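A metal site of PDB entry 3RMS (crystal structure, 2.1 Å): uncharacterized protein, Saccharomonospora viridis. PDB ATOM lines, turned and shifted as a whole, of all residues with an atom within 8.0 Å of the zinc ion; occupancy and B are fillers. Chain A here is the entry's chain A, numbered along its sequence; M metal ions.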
ATOM      1  N   TRP A   9     -28.014  21.053   9.277  1.00  0.00           N
ATOM      2  CA  TRP A   9     -26.940  21.726   8.578  1.00  0.00           C
ATOM      3  C   TRP A   9     -27.432  22.979   7.821  1.00  0.00           C
ATOM      4  O   TRP A   9     -28.558  22.992   7.312  1.00  0.00           O
ATOM      5  CB  TRP A   9     -26.291  20.792   7.587  1.00  0.00           C
ATOM      6  CG  TRP A   9     -25.572  19.655   8.276  1.00  0.00           C
ATOM      7  CD1 TRP A   9     -26.125  18.452   8.690  1.00  0.00           C
ATOM      8  CD2 TRP A   9     -24.193  19.626   8.682  1.00  0.00           C
ATOM      9  NE1 TRP A   9     -25.169  17.674   9.286  1.00  0.00           N
ATOM     10  CE2 TRP A   9     -23.974  18.360   9.307  1.00  0.00           C
ATOM     11  CE3 TRP A   9     -23.131  20.524   8.566  1.00  0.00           C
ATOM     12  CZ2 TRP A   9     -22.718  17.983   9.821  1.00  0.00           C
ATOM     13  CZ3 TRP A   9     -21.878  20.133   9.078  1.00  0.00           C
ATOM     14  CH2 TRP A   9     -21.687  18.868   9.680  1.00  0.00           C
ATOM     15  N   GLN A  10     -26.563  23.987   7.693  1.00  0.00           N
ATOM     16  CA  GLN A  10     -26.917  25.161   6.913  1.00  0.00           C
ATOM     17  C   GLN A  10     -25.613  25.822   6.468  1.00  0.00           C
ATOM     18  O   GLN A  10     -24.747  26.144   7.309  1.00  0.00           O
ATOM     19  CB  GLN A  10     -27.780  26.123   7.752  1.00  0.00           C
ATOM     20  CG  GLN A  10     -28.063  27.465   7.095  1.00  0.00           C
ATOM     21  CD  GLN A  10     -28.856  27.322   5.783  1.00  0.00           C
ATOM     22  OE1 GLN A  10     -29.893  26.669   5.734  1.00  0.00           O
ATOM     23  NE2 GLN A  10     -28.326  27.892   4.723  1.00  0.00           N
ATOM     24  N   ALA A  12     -23.385  28.842   5.191  1.00  0.00           N
ATOM     25  CA  ALA A  12     -23.389  30.284   5.402  1.00  0.00           C
ATOM     26  C   ALA A  12     -21.930  30.700   5.699  1.00  0.00           C
ATOM     27  O   ALA A  12     -21.147  29.922   6.308  1.00  0.00           O
ATOM     28  CB  ALA A  12     -24.326  30.682   6.560  1.00  0.00           C
ATOM     29  N   LYS A  15     -18.961  28.138   4.893  1.00  0.00           N
ATOM     30  CA  LYS A  15     -18.843  26.777   5.456  1.00  0.00           C
ATOM     31  C   LYS A  15     -20.218  26.183   5.694  1.00  0.00           C
ATOM     32  O   LYS A  15     -21.167  26.908   5.859  1.00  0.00           O
ATOM     33  CB  LYS A  15     -18.048  26.779   6.793  1.00  0.00           C
ATOM     34  CG  LYS A  15     -16.564  27.290   6.688  1.00  0.00           C
ATOM     35  CD  LYS A  15     -15.775  26.248   5.873  1.00  0.00           C
ATOM     36  CE  LYS A  15     -14.327  26.615   5.555  1.00  0.00           C
ATOM     37  NZ  LYS A  15     -13.695  25.489   4.759  1.00  0.00           N
ATOM     38  N   ARG A  16     -20.323  24.851   5.709  1.00  0.00           N
ATOM     39  CA  ARG A  16     -21.550  24.244   6.174  1.00  0.00           C
ATOM     40  C   ARG A  16     -21.515  24.130   7.714  1.00  0.00           C
ATOM     41  O   ARG A  16     -20.816  23.309   8.284  1.00  0.00           O
ATOM     42  CB  ARG A  16     -21.778  22.896   5.493  1.00  0.00           C
ATOM     43  CG  ARG A  16     -23.230  22.568   5.312  1.00  0.00           C
ATOM     44  CD  ARG A  16     -23.437  21.130   4.811  1.00  0.00           C
ATOM     45  NE  ARG A  16     -22.957  21.003   3.440  1.00  0.00           N
ATOM     46  CZ  ARG A  16     -23.072  19.915   2.677  1.00  0.00           C
ATOM     47  NH1 ARG A  16     -23.670  18.819   3.138  1.00  0.00           N
ATOM     48  NH2 ARG A  16     -22.590  19.946   1.451  1.00  0.00           N
ATOM     49  N   HIS A  17     -22.277  24.987   8.371  1.00  0.00           N
ATOM     50  CA  HIS A  17     -22.362  24.996   9.829  1.00  0.00           C
ATOM     51  C   HIS A  17     -23.583  24.145  10.240  1.00  0.00           C
ATOM     52  O   HIS A  17     -24.359  23.695   9.392  1.00  0.00           O
ATOM     53  CB  HIS A  17     -22.519  26.432  10.343  1.00  0.00           C
ATOM     54  CG  HIS A  17     -21.319  27.315  10.081  1.00  0.00           C
ATOM     55  ND1 HIS A  17     -20.258  27.414  10.969  1.00  0.00           N
ATOM     56  CD2 HIS A  17     -21.025  28.161   9.054  1.00  0.00           C
ATOM     57  CE1 HIS A  17     -19.358  28.243  10.478  1.00  0.00           C
ATOM     58  NE2 HIS A  17     -19.808  28.734   9.334  1.00  0.00           N
ATOM     59  N   VAL A  18     -23.722  23.893  11.530  1.00  0.00           N
ATOM     60  CA  VAL A  18     -24.904  23.258  12.099  1.00  0.00           C
ATOM     61  C   VAL A  18     -25.626  24.278  12.984  1.00  0.00           C
ATOM     62  O   VAL A  18     -24.974  25.136  13.622  1.00  0.00           O
ATOM     63  CB  VAL A  18     -24.520  22.003  12.962  1.00  0.00           C
ATOM     64  CG1 VAL A  18     -25.748  21.409  13.645  1.00  0.00           C
ATOM     65  CG2 VAL A  18     -23.819  20.954  12.113  1.00  0.00           C
ATOM     66  N   TYR A  19     -26.945  24.175  13.077  1.00  0.00           N
ATOM     67  CA  TYR A  19     -27.685  25.044  13.985  1.00  0.00           C
ATOM     68  C   TYR A  19     -28.772  24.281  14.732  1.00  0.00           C
ATOM     69  O   TYR A  19     -29.229  23.226  14.308  1.00  0.00           O
ATOM     70  CB  TYR A  19     -28.302  26.250  13.246  1.00  0.00           C
ATOM     71  CG  TYR A  19     -29.531  25.927  12.419  1.00  0.00           C
ATOM     72  CD1 TYR A  19     -30.805  26.164  12.924  1.00  0.00           C
ATOM     73  CD2 TYR A  19     -29.411  25.375  11.135  1.00  0.00           C
ATOM     74  CE1 TYR A  19     -31.925  25.874  12.171  1.00  0.00           C
ATOM     75  CE2 TYR A  19     -30.534  25.065  10.367  1.00  0.00           C
ATOM     76  CZ  TYR A  19     -31.777  25.314  10.897  1.00  0.00           C
ATOM     77  OH  TYR A  19     -32.890  25.029  10.149  1.00  0.00           O
ATOM     78  N   PHE A  32     -27.785  33.937  11.936  1.00  0.00           N
ATOM     79  CA  PHE A  32     -28.081  32.952  12.972  1.00  0.00           C
ATOM     80  C   PHE A  32     -26.764  32.552  13.642  1.00  0.00           C
ATOM     81  O   PHE A  32     -25.706  32.778  13.067  1.00  0.00           O
ATOM     82  CB  PHE A  32     -28.834  31.736  12.422  1.00  0.00           C
ATOM     83  CG  PHE A  32     -28.000  30.843  11.554  1.00  0.00           C
ATOM     84  CD1 PHE A  32     -27.250  29.801  12.105  1.00  0.00           C
ATOM     85  CD2 PHE A  32     -27.976  31.006  10.175  1.00  0.00           C
ATOM     86  CE1 PHE A  32     -26.485  28.966  11.305  1.00  0.00           C
ATOM     87  CE2 PHE A  32     -27.218  30.188   9.369  1.00  0.00           C
ATOM     88  CZ  PHE A  32     -26.471  29.161   9.929  1.00  0.00           C
ATOM     89  N   THR A  33     -26.839  31.988  14.853  1.00  0.00           N
ATOM     90  CA  THR A  33     -25.635  31.568  15.535  1.00  0.00           C
ATOM     91  C   THR A  33     -25.539  30.041  15.443  1.00  0.00           C
ATOM     92  O   THR A  33     -26.441  29.298  15.888  1.00  0.00           O
ATOM     93  CB  THR A  33     -25.635  32.046  16.988  1.00  0.00           C
ATOM     94  OG1 THR A  33     -25.779  33.463  16.983  1.00  0.00           O
ATOM     95  CG2 THR A  33     -24.345  31.652  17.725  1.00  0.00           C
ATOM     96  N   ALA A  34     -24.460  29.580  14.861  1.00  0.00           N
ATOM     97  CA  ALA A  34     -24.244  28.151  14.628  1.00  0.00           C
ATOM     98  C   ALA A  34     -23.757  27.452  15.934  1.00  0.00           C
ATOM     99  O   ALA A  34     -23.575  28.110  16.966  1.00  0.00           O
ATOM    100  CB  ALA A  34     -23.279  27.966  13.528  1.00  0.00           C
ATOM    101  N   LEU A  35     -23.590  26.128  15.912  1.00  0.00           N
ATOM    102  CA  LEU A  35     -23.131  25.409  17.120  1.00  0.00           C
ATOM    103  C   LEU A  35     -21.745  25.874  17.520  1.00  0.00           C
ATOM    104  O   LEU A  35     -21.459  25.970  18.693  1.00  0.00           O
ATOM    105  CB  LEU A  35     -23.087  23.890  16.934  1.00  0.00           C
ATOM    106  CG  LEU A  35     -24.401  23.139  16.884  1.00  0.00           C
ATOM    107  CD1 LEU A  35     -24.081  21.624  16.834  1.00  0.00           C
ATOM    108  CD2 LEU A  35     -25.272  23.503  18.086  1.00  0.00           C
ATOM    109  N   CYS A  36     -20.890  26.153  16.542  1.00  0.00           N
ATOM    110  CA  CYS A  36     -19.572  26.681  16.831  1.00  0.00           C
ATOM    111  C   CYS A  36     -19.605  28.064  17.451  1.00  0.00           C
ATOM    112  O   CYS A  36     -18.573  28.582  17.817  1.00  0.00           O
ATOM    113  CB  CYS A  36     -18.735  26.718  15.559  1.00  0.00           C
ATOM    114  SG  CYS A  36     -19.355  27.885  14.302  1.00  0.00           S
ATOM    115  N   GLY A  37     -20.783  28.703  17.539  1.00  0.00           N
ATOM    116  CA  GLY A  37     -20.871  30.031  18.169  1.00  0.00           C
ATOM    117  C   GLY A  37     -20.592  31.193  17.209  1.00  0.00           C
ATOM    118  O   GLY A  37     -20.621  32.368  17.588  1.00  0.00           O
ATOM    119  N   GLU A  38     -20.320  30.890  15.939  1.00  0.00           N
ATOM    120  CA  GLU A  38     -20.110  31.959  14.969  1.00  0.00           C
ATOM    121  C   GLU A  38     -21.468  32.443  14.480  1.00  0.00           C
ATOM    122  O   GLU A  38     -22.371  31.653  14.278  1.00  0.00           O
ATOM    123  CB  GLU A  38     -19.234  31.473  13.806  1.00  0.00           C
ATOM    124  CG  GLU A  38     -18.699  32.608  12.903  1.00  0.00           C
ATOM    125  CD  GLU A  38     -17.660  33.517  13.621  1.00  0.00           C
ATOM    126  OE1 GLU A  38     -17.734  34.775  13.452  1.00  0.00           O
ATOM    127  OE2 GLU A  38     -16.781  32.988  14.355  1.00  0.00           O
ATOM    128  N   THR A  39     -21.623  33.762  14.318  1.00  0.00           N
ATOM    129  CA  THR A  39     -22.854  34.358  13.822  1.00  0.00           C
ATOM    130  C   THR A  39     -22.635  34.534  12.330  1.00  0.00           C
ATOM    131  O   THR A  39     -21.684  35.185  11.894  1.00  0.00           O
ATOM    132  CB  THR A  39     -23.157  35.728  14.519  1.00  0.00           C
ATOM    133  OG1 THR A  39     -23.265  35.515  15.922  1.00  0.00           O
ATOM    134  CG2 THR A  39     -24.445  36.352  14.012  1.00  0.00           C
ATOM    135  N   VAL A  40     -23.517  33.925  11.549  1.00  0.00           N
ATOM    136  CA  VAL A  40     -23.321  33.809  10.113  1.00  0.00           C
ATOM    137  C   VAL A  40     -24.622  34.144   9.410  1.00  0.00           C
ATOM    138  O   VAL A  40     -25.695  33.923   9.959  1.00  0.00           O
ATOM    139  CB  VAL A  40     -22.881  32.359   9.741  1.00  0.00           C
ATOM    140  CG1 VAL A  40     -21.503  32.077  10.270  1.00  0.00           C
ATOM    141  CG2 VAL A  40     -23.874  31.350  10.286  1.00  0.00           C
ATOM    142  N   GLU A  58     -17.361  21.560   5.263  1.00  0.00           N
ATOM    143  CA  GLU A  58     -18.055  21.583   6.558  1.00  0.00           C
ATOM    144  C   GLU A  58     -17.257  22.390   7.578  1.00  0.00           C
ATOM    145  O   GLU A  58     -16.014  22.444   7.557  1.00  0.00           O
ATOM    146  CB  GLU A  58     -18.315  20.166   7.074  1.00  0.00           C
ATOM    147  CG  GLU A  58     -18.574  19.175   5.978  1.00  0.00           C
ATOM    148  CD  GLU A  58     -17.333  18.399   5.616  1.00  0.00           C
ATOM    149  OE1 GLU A  58     -16.938  17.484   6.410  1.00  0.00           O
ATOM    150  OE2 GLU A  58     -16.730  18.720   4.557  1.00  0.00           O
ATOM    151  N   CYS A  59     -17.991  23.071   8.454  1.00  0.00           N
ATOM    152  CA  CYS A  59     -17.377  23.731   9.593  1.00  0.00           C
ATOM    153  C   CYS A  59     -16.875  22.640  10.579  1.00  0.00           C
ATOM    154  O   CYS A  59     -17.669  21.916  11.174  1.00  0.00           O
ATOM    155  CB  CYS A  59     -18.385  24.616  10.293  1.00  0.00           C
ATOM    156  SG  CYS A  59     -17.784  25.319  11.872  1.00  0.00           S
ATOM    157  N   PRO A  60     -15.542  22.545  10.746  1.00  0.00           N
ATOM    158  CA  PRO A  60     -14.970  21.500  11.631  1.00  0.00           C
ATOM    159  C   PRO A  60     -15.477  21.582  13.086  1.00  0.00           C
ATOM    160  O   PRO A  60     -15.703  20.542  13.679  1.00  0.00           O
ATOM    161  CB  PRO A  60     -13.457  21.761  11.568  1.00  0.00           C
ATOM    162  CG  PRO A  60     -13.238  22.536  10.264  1.00  0.00           C
ATOM    163  CD  PRO A  60     -14.488  23.388  10.134  1.00  0.00           C
ATOM    164  N   VAL A  61     -15.643  22.783  13.637  1.00  0.00           N
ATOM    165  CA  VAL A  61     -16.099  22.929  15.000  1.00  0.00           C
ATOM    166  C   VAL A  61     -17.546  22.491  15.156  1.00  0.00           C
ATOM    167  O   VAL A  61     -17.861  21.818  16.114  1.00  0.00           O
ATOM    168  CB  VAL A  61     -15.917  24.380  15.558  1.00  0.00           C
ATOM    169  CG1 VAL A  61     -16.429  24.464  16.997  1.00  0.00           C
ATOM    170  CG2 VAL A  61     -14.444  24.826  15.475  1.00  0.00           C
ATOM    171  N   CYS A  62     -18.415  22.907  14.231  1.00  0.00           N
ATOM    172  CA  CYS A  62     -19.807  22.441  14.187  1.00  0.00           C
ATOM    173  C   CYS A  62     -19.926  20.919  14.024  1.00  0.00           C
ATOM    174  O   CYS A  62     -20.773  20.301  14.620  1.00  0.00           O
ATOM    175  CB  CYS A  62     -20.590  23.116  13.042  1.00  0.00           C
ATOM    176  SG  CYS A  62     -21.208  24.817  13.469  1.00  0.00           S
ATOM    177  N   THR A  63     -19.104  20.341  13.161  1.00  0.00           N
ATOM    178  CA  THR A  63     -19.148  18.906  12.909  1.00  0.00           C
ATOM    179  C   THR A  63     -18.865  18.134  14.171  1.00  0.00           C
ATOM    180  O   THR A  63     -19.632  17.258  14.554  1.00  0.00           O
ATOM    181  CB  THR A  63     -18.133  18.483  11.830  1.00  0.00           C
ATOM    182  OG1 THR A  63     -18.456  19.145  10.597  1.00  0.00           O
ATOM    183  CG2 THR A  63     -18.152  17.017  11.615  1.00  0.00           C
ATOM    184  N   ALA A  65     -18.965  19.245  17.204  1.00  0.00           N
ATOM    185  CA  ALA A  65     -19.968  19.617  18.205  1.00  0.00           C
ATOM    186  C   ALA A  65     -21.274  18.859  17.996  1.00  0.00           C
ATOM    187  O   ALA A  65     -21.898  18.420  18.968  1.00  0.00           O
ATOM    188  CB  ALA A  65     -20.209  21.122  18.180  1.00  0.00           C
ATOM    189  N   LEU A  90      -9.205  27.347  15.472  1.00  0.00           N
ATOM    190  CA  LEU A  90     -10.204  26.285  15.498  1.00  0.00           C
ATOM    191  C   LEU A  90     -10.131  25.466  16.811  1.00  0.00           C
ATOM    192  O   LEU A  90     -11.160  25.166  17.402  1.00  0.00           O
ATOM    193  CB  LEU A  90     -10.082  25.369  14.269  1.00  0.00           C
ATOM    194  CG  LEU A  90     -10.494  25.934  12.903  1.00  0.00           C
ATOM    195  CD1 LEU A  90     -10.032  25.010  11.798  1.00  0.00           C
ATOM    196  CD2 LEU A  90     -11.981  26.174  12.794  1.00  0.00           C
ATOM    197  N   ARG A  93     -11.676  27.613  19.708  1.00  0.00           N
ATOM    198  CA  ARG A  93     -13.120  27.681  19.620  1.00  0.00           C
ATOM    199  C   ARG A  93     -13.763  26.363  19.996  1.00  0.00           C
ATOM    200  O   ARG A  93     -14.761  26.358  20.694  1.00  0.00           O
ATOM    201  CB  ARG A  93     -13.555  28.054  18.187  1.00  0.00           C
ATOM    202  CG  ARG A  93     -15.060  28.240  18.079  1.00  0.00           C
ATOM    203  CD  ARG A  93     -15.556  29.357  19.013  1.00  0.00           C
ATOM    204  NE  ARG A  93     -15.068  30.690  18.613  1.00  0.00           N
ATOM    205  CZ  ARG A  93     -15.614  31.439  17.643  1.00  0.00           C
ATOM    206  NH1 ARG A  93     -16.670  31.010  16.966  1.00  0.00           N
ATOM    207  NH2 ARG A  93     -15.098  32.622  17.355  1.00  0.00           N
ATOM    208  N   VAL A  97     -16.428  25.482  22.956  1.00  0.00           N
ATOM    209  CA  VAL A  97     -17.706  24.827  22.684  1.00  0.00           C
ATOM    210  C   VAL A  97     -17.888  23.516  23.475  1.00  0.00           C
ATOM    211  O   VAL A  97     -18.940  23.233  24.020  1.00  0.00           O
ATOM    212  CB  VAL A  97     -17.860  24.598  21.124  1.00  0.00           C
ATOM    213  CG1 VAL A  97     -19.158  23.870  20.815  1.00  0.00           C
ATOM    214  CG2 VAL A  97     -17.827  25.944  20.376  1.00  0.00           C
HETATM  215 ZN    ZN M   1     -19.712  26.283  12.654  1.00  0.00          ZN
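The side-chain sulfur of Cys 62 lies close to the backbone NH of Leu 35 (3.7 Å). SG of Cys 62 lies close to N of Val 18 (3.3 Å). The side-chain hydroxyl (OG1) of Thr 63 lies within hydrogen-bond range of the backbone carbonyl oxygen (O) of Cys 59 (2.9 Å). SG of Cys 36 lies close to N of Glu 38 (3.6 Å). The backbone NH (N) of Gln 10 lies within hydrogen-bond range of the backbone carbonyl oxygen (O) of His 17, 2.8 Å away. N of Cys 59 lies within hydrogen-bond range of O of Arg 16 (2.8 Å). The side-chain sulfur (SG) of Cys 59 lies close to the backbone NH (N) of Val 61 (3.8 Å). The guanidinium group (NH1) of Arg 93 sits at hydrogen-bond distance from the backbone carbonyl oxygen (O) of Cys 36, at 3.2 Å.
ND1 of His 17 is bound to the zinc ion (2.1 Å). SG of Cys 62 binds the zinc ion. The side-chain sulfur (SG) of Cys 59 is bound to the zinc ion (2.3 Å). SG of Cys 36 binds the zinc ion, 2.3 Å away. The zinc ion has four donor atoms within binding distance.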
